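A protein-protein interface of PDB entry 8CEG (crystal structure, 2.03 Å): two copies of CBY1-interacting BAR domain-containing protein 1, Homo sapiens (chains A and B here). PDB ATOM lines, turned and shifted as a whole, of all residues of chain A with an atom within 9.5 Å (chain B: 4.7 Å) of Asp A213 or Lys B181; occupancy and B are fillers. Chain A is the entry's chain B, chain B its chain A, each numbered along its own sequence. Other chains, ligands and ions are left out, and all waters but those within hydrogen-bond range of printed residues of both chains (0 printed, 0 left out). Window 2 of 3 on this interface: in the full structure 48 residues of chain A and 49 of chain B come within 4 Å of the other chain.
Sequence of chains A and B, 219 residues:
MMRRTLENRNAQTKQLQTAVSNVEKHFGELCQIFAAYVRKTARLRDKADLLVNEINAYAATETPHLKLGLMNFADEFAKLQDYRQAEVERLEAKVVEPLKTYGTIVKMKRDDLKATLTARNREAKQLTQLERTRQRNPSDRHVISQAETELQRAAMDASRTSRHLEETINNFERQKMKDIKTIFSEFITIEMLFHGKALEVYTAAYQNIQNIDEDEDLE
CD1 of Ile B180 touches OH of Tyr A58, 2.9 Å away.
Ser B185 touches Ile A209.
Asp A213 touches one residue of chain B.
Printed residues of chain A within 4 Å of Lys B181: Gln A210 and Asp A213.
Of the printed residues of chain A, Ile B180 touches Tyr A58 (2.9 Å).
Of the printed residues of chain B, Tyr A58 touches Ile B180.
The nearest printed residue of chain A that does not touch Ser B185 is Tyr A206 (4.04 Å).
NZ of Lys B181 is in hydrogen-bond range of O of Gln A210 (3.1 Å).
The side-chain hydroxyl of Ser B185 is in hydrogen-bond range of the side-chain amide oxygen of Gln A210 (2.6 Å).
The side-chain amino group of Lys B181 is in salt-bridge range of the side-chain carboxylate of Asp A213 (2.9 Å).
Of the 9 printed residues of chain B, 3 touch a printed residue of chain A.
Hydrophobic or aromatic side chains of chain B that line the printed part of chain A: Ile B180.
Of the 17 printed residues of chain A, 4 touch a printed residue of chain B.
Along chain A the printed residues that touch a printed residue of chain B span positions 58 to 213.
Among the printed residues, 5 pairs touch across the chains.
Among the printed residues, Asp or Glu carboxylates within 4 Å of a Lys or Arg side-chain nitrogen of the other chain: Asp A213 with Lys B181 (2.9 Å).
No position is printed for both chains.
NE2 of Gln A210 lies within hydrogen-bond range of OH of Tyr A206 (3.4 Å).
The backbone carbonyl oxygen (O) of Lys B181 lies within hydrogen-bond range of the side-chain hydroxyl (OG) of Ser B185, 2.8 Å away.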
ATOM      1  N   TYR A  58      -8.053  11.022   3.922  1.00  0.00           N
ATOM      2  CA  TYR A  58      -9.133  10.037   3.998  1.00  0.00           C
ATOM      3  C   TYR A  58     -10.442  10.692   4.426  1.00  0.00           C
ATOM      4  O   TYR A  58     -11.496  10.396   3.863  1.00  0.00           O
ATOM      5  CB  TYR A  58      -8.743   8.909   4.954  1.00  0.00           C
ATOM      6  CG  TYR A  58      -9.883   7.983   5.297  1.00  0.00           C
ATOM      7  CD1 TYR A  58     -10.616   7.378   4.307  1.00  0.00           C
ATOM      8  CD2 TYR A  58     -10.217   7.730   6.623  1.00  0.00           C
ATOM      9  CE1 TYR A  58     -11.689   6.523   4.616  1.00  0.00           C
ATOM     10  CE2 TYR A  58     -11.243   6.912   6.949  1.00  0.00           C
ATOM     11  CZ  TYR A  58     -11.978   6.296   5.933  1.00  0.00           C
ATOM     12  OH  TYR A  58     -13.001   5.474   6.250  1.00  0.00           O
ATOM     13  N   THR A  63     -18.280  10.491   4.723  1.00  0.00           N
ATOM     14  CA  THR A  63     -19.600  11.017   5.017  1.00  0.00           C
ATOM     15  C   THR A  63     -19.503  12.065   6.126  1.00  0.00           C
ATOM     16  O   THR A  63     -18.580  12.038   6.926  1.00  0.00           O
ATOM     17  CB  THR A  63     -20.539   9.873   5.411  1.00  0.00           C
ATOM     18  OG1 THR A  63     -19.980   9.129   6.509  1.00  0.00           O
ATOM     19  CG2 THR A  63     -20.774   8.941   4.180  1.00  0.00           C
ATOM     20  N   HIS A  65     -20.436  13.205   9.247  1.00  0.00           N
ATOM     21  CA  HIS A  65     -20.081  13.049  10.659  1.00  0.00           C
ATOM     22  C   HIS A  65     -18.688  12.437  10.824  1.00  0.00           C
ATOM     23  O   HIS A  65     -17.908  12.839  11.712  1.00  0.00           O
ATOM     24  CB  HIS A  65     -21.163  12.188  11.318  1.00  0.00           C
ATOM     25  CG  HIS A  65     -21.422  12.494  12.764  1.00  0.00           C
ATOM     26  ND1 HIS A  65     -22.688  12.763  13.248  1.00  0.00           N
ATOM     27  CD2 HIS A  65     -20.596  12.520  13.840  1.00  0.00           C
ATOM     28  CE1 HIS A  65     -22.625  12.968  14.552  1.00  0.00           C
ATOM     29  NE2 HIS A  65     -21.365  12.835  14.936  1.00  0.00           N
ATOM     30  N   LEU A  66     -18.361  11.465   9.974  1.00  0.00           N
ATOM     31  CA  LEU A  66     -17.066  10.801  10.047  1.00  0.00           C
ATOM     32  C   LEU A  66     -15.958  11.731   9.570  1.00  0.00           C
ATOM     33  O   LEU A  66     -14.897  11.799  10.195  1.00  0.00           O
ATOM     34  CB  LEU A  66     -17.111   9.510   9.214  1.00  0.00           C
ATOM     35  CG  LEU A  66     -15.796   8.742   9.060  1.00  0.00           C
ATOM     36  CD1 LEU A  66     -15.231   8.413  10.417  1.00  0.00           C
ATOM     37  CD2 LEU A  66     -16.045   7.485   8.255  1.00  0.00           C
ATOM     38  N   LYS A  67     -16.224  12.501   8.510  1.00  0.00           N
ATOM     39  CA  LYS A  67     -15.260  13.478   8.021  1.00  0.00           C
ATOM     40  C   LYS A  67     -14.954  14.485   9.113  1.00  0.00           C
ATOM     41  O   LYS A  67     -13.788  14.815   9.372  1.00  0.00           O
ATOM     42  CB  LYS A  67     -15.830  14.201   6.789  1.00  0.00           C
ATOM     43  CG  LYS A  67     -15.099  15.498   6.356  1.00  0.00           C
ATOM     44  CD  LYS A  67     -15.787  16.293   5.201  1.00  0.00           C
ATOM     45  CE  LYS A  67     -15.694  15.631   3.829  1.00  0.00           C
ATOM     46  NZ  LYS A  67     -16.356  16.486   2.787  1.00  0.00           N
ATOM     47  N   GLY A  69     -15.269  14.252  12.410  1.00  0.00           N
ATOM     48  CA  GLY A  69     -14.508  13.683  13.513  1.00  0.00           C
ATOM     49  C   GLY A  69     -13.053  13.425  13.167  1.00  0.00           C
ATOM     50  O   GLY A  69     -12.152  13.627  13.999  1.00  0.00           O
ATOM     51  N   LEU A  70     -12.790  12.969  11.944  1.00  0.00           N
ATOM     52  CA  LEU A  70     -11.412  12.670  11.574  1.00  0.00           C
ATOM     53  C   LEU A  70     -10.591  13.938  11.368  1.00  0.00           C
ATOM     54  O   LEU A  70      -9.412  13.964  11.716  1.00  0.00           O
ATOM     55  CB  LEU A  70     -11.376  11.803  10.324  1.00  0.00           C
ATOM     56  CG  LEU A  70     -11.825  10.342  10.494  1.00  0.00           C
ATOM     57  CD1 LEU A  70     -11.898   9.701   9.132  1.00  0.00           C
ATOM     58  CD2 LEU A  70     -10.860   9.554  11.438  1.00  0.00           C
ATOM     59  N   ALA A 205      -8.829  14.498  22.289  1.00  0.00           N
ATOM     60  CA  ALA A 205      -9.003  13.718  21.066  1.00  0.00           C
ATOM     61  C   ALA A 205      -9.764  12.415  21.319  1.00  0.00           C
ATOM     62  O   ALA A 205     -10.574  11.991  20.487  1.00  0.00           O
ATOM     63  CB  ALA A 205      -7.641  13.425  20.436  1.00  0.00           C
ATOM     64  N   TYR A 206      -9.517  11.766  22.449  1.00  0.00           N
ATOM     65  CA  TYR A 206     -10.208  10.525  22.770  1.00  0.00           C
ATOM     66  C   TYR A 206     -11.720  10.749  22.868  1.00  0.00           C
ATOM     67  O   TYR A 206     -12.510  10.060  22.215  1.00  0.00           O
ATOM     68  CB  TYR A 206      -9.697   9.958  24.096  1.00  0.00           C
ATOM     69  CG  TYR A 206     -10.347   8.661  24.388  1.00  0.00           C
ATOM     70  CD1 TYR A 206      -9.934   7.511  23.725  1.00  0.00           C
ATOM     71  CD2 TYR A 206     -11.463   8.587  25.243  1.00  0.00           C
ATOM     72  CE1 TYR A 206     -10.600   6.299  23.927  1.00  0.00           C
ATOM     73  CE2 TYR A 206     -12.133   7.386  25.446  1.00  0.00           C
ATOM     74  CZ  TYR A 206     -11.688   6.252  24.806  1.00  0.00           C
ATOM     75  OH  TYR A 206     -12.327   5.068  25.040  1.00  0.00           O
ATOM     76  N   GLN A 207     -12.122  11.765  23.645  1.00  0.00           N
ATOM     77  CA  GLN A 207     -13.532  12.027  23.898  1.00  0.00           C
ATOM     78  C   GLN A 207     -14.243  12.294  22.593  1.00  0.00           C
ATOM     79  O   GLN A 207     -15.404  11.885  22.409  1.00  0.00           O
ATOM     80  CB  GLN A 207     -13.699  13.224  24.825  1.00  0.00           C
ATOM     81  CG  GLN A 207     -13.202  12.948  26.179  1.00  0.00           C
ATOM     82  CD  GLN A 207     -13.548  14.022  27.184  1.00  0.00           C
ATOM     83  OE1 GLN A 207     -14.642  14.032  27.736  1.00  0.00           O
ATOM     84  NE2 GLN A 207     -12.582  14.921  27.463  1.00  0.00           N
ATOM     85  N   ASN A 208     -13.564  13.023  21.696  1.00  0.00           N
ATOM     86  CA  ASN A 208     -14.163  13.399  20.428  1.00  0.00           C
ATOM     87  C   ASN A 208     -14.208  12.262  19.416  1.00  0.00           C
ATOM     88  O   ASN A 208     -15.211  12.132  18.718  1.00  0.00           O
ATOM     89  CB  ASN A 208     -13.398  14.564  19.814  1.00  0.00           C
ATOM     90  CG  ASN A 208     -13.623  15.861  20.565  1.00  0.00           C
ATOM     91  OD1 ASN A 208     -14.657  16.047  21.207  1.00  0.00           O
ATOM     92  ND2 ASN A 208     -12.667  16.780  20.466  1.00  0.00           N
ATOM     93  N   ILE A 209     -13.187  11.388  19.360  1.00  0.00           N
ATOM     94  CA  ILE A 209     -13.273  10.222  18.480  1.00  0.00           C
ATOM     95  C   ILE A 209     -14.460   9.346  18.871  1.00  0.00           C
ATOM     96  O   ILE A 209     -15.071   8.707  18.015  1.00  0.00           O
ATOM     97  CB  ILE A 209     -11.979   9.390  18.481  1.00  0.00           C
ATOM     98  CG1 ILE A 209     -10.886  10.039  17.628  1.00  0.00           C
ATOM     99  CG2 ILE A 209     -12.215   8.009  17.910  1.00  0.00           C
ATOM    100  CD1 ILE A 209     -11.085   9.823  16.123  1.00  0.00           C
ATOM    101  N   GLN A 210     -14.791   9.287  20.160  1.00  0.00           N
ATOM    102  CA  GLN A 210     -15.845   8.388  20.610  1.00  0.00           C
ATOM    103  C   GLN A 210     -17.230   8.837  20.117  1.00  0.00           C
ATOM    104  O   GLN A 210     -18.106   7.994  19.910  1.00  0.00           O
ATOM    105  CB  GLN A 210     -15.763   8.282  22.122  1.00  0.00           C
ATOM    106  CG  GLN A 210     -14.463   7.542  22.568  1.00  0.00           C
ATOM    107  CD  GLN A 210     -14.538   6.067  22.286  1.00  0.00           C
ATOM    108  OE1 GLN A 210     -14.051   5.569  21.299  1.00  0.00           O
ATOM    109  NE2 GLN A 210     -15.179   5.371  23.144  1.00  0.00           N
ATOM    110  N   ASN A 211     -17.436  10.128  19.855  1.00  0.00           N
ATOM    111  CA  ASN A 211     -18.707  10.607  19.322  1.00  0.00           C
ATOM    112  C   ASN A 211     -18.758  10.527  17.798  1.00  0.00           C
ATOM    113  O   ASN A 211     -19.659  11.099  17.181  1.00  0.00           O
ATOM    114  CB  ASN A 211     -18.945  12.069  19.709  1.00  0.00           C
ATOM    115  CG  ASN A 211     -19.127  12.269  21.191  1.00  0.00           C
ATOM    116  OD1 ASN A 211     -20.052  11.741  21.805  1.00  0.00           O
ATOM    117  ND2 ASN A 211     -18.284  13.104  21.760  1.00  0.00           N
ATOM    118  N   ILE A 212     -17.833   9.802  17.189  1.00  0.00           N
ATOM    119  CA  ILE A 212     -17.799   9.712  15.740  1.00  0.00           C
ATOM    120  C   ILE A 212     -18.977   8.908  15.194  1.00  0.00           C
ATOM    121  O   ILE A 212     -19.496   9.220  14.119  1.00  0.00           O
ATOM    122  CB  ILE A 212     -16.445   9.136  15.296  1.00  0.00           C
ATOM    123  CG1 ILE A 212     -15.965   9.859  14.043  1.00  0.00           C
ATOM    124  CG2 ILE A 212     -16.506   7.594  15.127  1.00  0.00           C
ATOM    125  CD1 ILE A 212     -14.569   9.497  13.666  1.00  0.00           C
ATOM    126  N   ASP A 213     -19.390   7.844  15.890  1.00  0.00           N
ATOM    127  CA  ASP A 213     -20.483   7.026  15.370  1.00  0.00           C
ATOM    128  C   ASP A 213     -21.855   7.671  15.579  1.00  0.00           C
ATOM    129  O   ASP A 213     -22.851   7.118  15.110  1.00  0.00           O
ATOM    130  CB  ASP A 213     -20.434   5.600  15.965  1.00  0.00           C
ATOM    131  CG  ASP A 213     -20.386   5.567  17.498  1.00  0.00           C
ATOM    132  OD1 ASP A 213     -20.364   6.636  18.157  1.00  0.00           O
ATOM    133  OD2 ASP A 213     -20.369   4.438  18.044  1.00  0.00           O
ATOM    134  N   GLU A 214     -21.931   8.830  16.240  1.00  0.00           N
ATOM    135  CA  GLU A 214     -23.214   9.483  16.529  1.00  0.00           C
ATOM    136  C   GLU A 214     -23.971   9.834  15.236  1.00  0.00           C
ATOM    137  O   GLU A 214     -23.540   9.491  14.120  1.00  0.00           O
ATOM    138  CB  GLU A 214     -22.997  10.750  17.374  1.00  0.00           C
ATOM    139  N   MET B 177     -16.934   1.934  10.123  1.00  0.00           N
ATOM    140  CA  MET B 177     -17.028   2.954  11.160  1.00  0.00           C
ATOM    141  C   MET B 177     -16.639   2.402  12.516  1.00  0.00           C
ATOM    142  O   MET B 177     -15.936   3.066  13.292  1.00  0.00           O
ATOM    143  CB  MET B 177     -18.450   3.481  11.267  1.00  0.00           C
ATOM    144  CG  MET B 177     -18.603   4.600  12.326  1.00  0.00           C
ATOM    145  SD  MET B 177     -18.683   6.185  11.553  1.00  0.00           S
ATOM    146  CE  MET B 177     -20.113   5.817  10.499  1.00  0.00           C
ATOM    147  N   LYS B 178     -17.129   1.208  12.843  1.00  0.00           N
ATOM    148  CA  LYS B 178     -16.756   0.593  14.111  1.00  0.00           C
ATOM    149  C   LYS B 178     -15.253   0.412  14.187  1.00  0.00           C
ATOM    150  O   LYS B 178     -14.649   0.648  15.230  1.00  0.00           O
ATOM    151  CB  LYS B 178     -17.447  -0.763  14.302  1.00  0.00           C
ATOM    152  CG  LYS B 178     -18.671  -0.695  15.228  1.00  0.00           C
ATOM    153  CD  LYS B 178     -18.908  -2.001  16.019  1.00  0.00           C
ATOM    154  CE  LYS B 178     -20.246  -1.951  16.804  1.00  0.00           C
ATOM    155  NZ  LYS B 178     -21.466  -2.001  15.918  1.00  0.00           N
ATOM    156  N   ASP B 179     -14.657  -0.024  13.086  1.00  0.00           N
ATOM    157  CA  ASP B 179     -13.254  -0.358  13.056  1.00  0.00           C
ATOM    158  C   ASP B 179     -12.411   0.893  13.118  1.00  0.00           C
ATOM    159  O   ASP B 179     -11.399   0.916  13.828  1.00  0.00           O
ATOM    160  CB  ASP B 179     -12.915  -1.164  11.809  1.00  0.00           C
ATOM    161  CG  ASP B 179     -13.325  -2.638  11.924  1.00  0.00           C
ATOM    162  OD1 ASP B 179     -13.640  -3.131  13.046  1.00  0.00           O
ATOM    163  OD2 ASP B 179     -13.301  -3.313  10.867  1.00  0.00           O
ATOM    164  N   ILE B 180     -12.815   1.943  12.386  1.00  0.00           N
ATOM    165  CA  ILE B 180     -12.093   3.212  12.461  1.00  0.00           C
ATOM    166  C   ILE B 180     -12.130   3.759  13.875  1.00  0.00           C
ATOM    167  O   ILE B 180     -11.137   4.302  14.376  1.00  0.00           O
ATOM    168  CB  ILE B 180     -12.692   4.260  11.508  1.00  0.00           C
ATOM    169  CG1 ILE B 180     -12.235   4.024  10.099  1.00  0.00           C
ATOM    170  CG2 ILE B 180     -12.278   5.729  11.915  1.00  0.00           C
ATOM    171  CD1 ILE B 180     -13.122   4.793   9.082  1.00  0.00           C
ATOM    172  N   LYS B 181     -13.291   3.689  14.515  1.00  0.00           N
ATOM    173  CA  LYS B 181     -13.392   4.176  15.883  1.00  0.00           C
ATOM    174  C   LYS B 181     -12.475   3.371  16.811  1.00  0.00           C
ATOM    175  O   LYS B 181     -11.797   3.947  17.667  1.00  0.00           O
ATOM    176  CB  LYS B 181     -14.869   4.138  16.307  1.00  0.00           C
ATOM    177  CG  LYS B 181     -15.174   4.444  17.799  1.00  0.00           C
ATOM    178  CD  LYS B 181     -16.712   4.576  18.092  1.00  0.00           C
ATOM    179  CE  LYS B 181     -16.977   4.526  19.637  1.00  0.00           C
ATOM    180  NZ  LYS B 181     -18.378   4.890  20.066  1.00  0.00           N
ATOM    181  N   THR B 182     -12.430   2.042  16.636  1.00  0.00           N
ATOM    182  CA  THR B 182     -11.615   1.179  17.485  1.00  0.00           C
ATOM    183  C   THR B 182     -10.144   1.480  17.298  1.00  0.00           C
ATOM    184  O   THR B 182      -9.402   1.613  18.267  1.00  0.00           O
ATOM    185  CB  THR B 182     -11.897  -0.295  17.174  1.00  0.00           C
ATOM    186  OG1 THR B 182     -13.286  -0.570  17.410  1.00  0.00           O
ATOM    187  CG2 THR B 182     -11.044  -1.228  18.038  1.00  0.00           C
ATOM    188  N   ILE B 183      -9.719   1.615  16.047  1.00  0.00           N
ATOM    189  CA  ILE B 183      -8.312   1.716  15.732  1.00  0.00           C
ATOM    190  C   ILE B 183      -7.745   3.044  16.208  1.00  0.00           C
ATOM    191  O   ILE B 183      -6.658   3.081  16.775  1.00  0.00           O
ATOM    192  CB  ILE B 183      -8.107   1.491  14.231  1.00  0.00           C
ATOM    193  CG1 ILE B 183      -8.325  -0.002  13.928  1.00  0.00           C
ATOM    194  CG2 ILE B 183      -6.734   1.943  13.807  1.00  0.00           C
ATOM    195  CD1 ILE B 183      -8.579  -0.297  12.472  1.00  0.00           C
ATOM    196  N   PHE B 184      -8.460   4.139  15.976  1.00  0.00           N
ATOM    197  CA  PHE B 184      -8.021   5.438  16.450  1.00  0.00           C
ATOM    198  C   PHE B 184      -8.193   5.555  17.944  1.00  0.00           C
ATOM    199  O   PHE B 184      -7.359   6.176  18.597  1.00  0.00           O
ATOM    200  CB  PHE B 184      -8.775   6.549  15.722  1.00  0.00           C
ATOM    201  CG  PHE B 184      -8.239   6.803  14.361  1.00  0.00           C
ATOM    202  CD1 PHE B 184      -8.612   6.007  13.281  1.00  0.00           C
ATOM    203  CD2 PHE B 184      -7.351   7.813  14.150  1.00  0.00           C
ATOM    204  CE1 PHE B 184      -8.081   6.250  12.017  1.00  0.00           C
ATOM    205  CE2 PHE B 184      -6.817   8.057  12.895  1.00  0.00           C
ATOM    206  CZ  PHE B 184      -7.181   7.290  11.830  1.00  0.00           C
ATOM    207  N   SER B 185      -9.197   4.884  18.516  1.00  0.00           N
ATOM    208  CA  SER B 185      -9.333   4.912  19.968  1.00  0.00           C
ATOM    209  C   SER B 185      -8.196   4.156  20.644  1.00  0.00           C
ATOM    210  O   SER B 185      -7.695   4.611  21.675  1.00  0.00           O
ATOM    211  CB  SER B 185     -10.671   4.337  20.399  1.00  0.00           C
ATOM    212  OG  SER B 185     -11.711   5.236  20.117  1.00  0.00           O
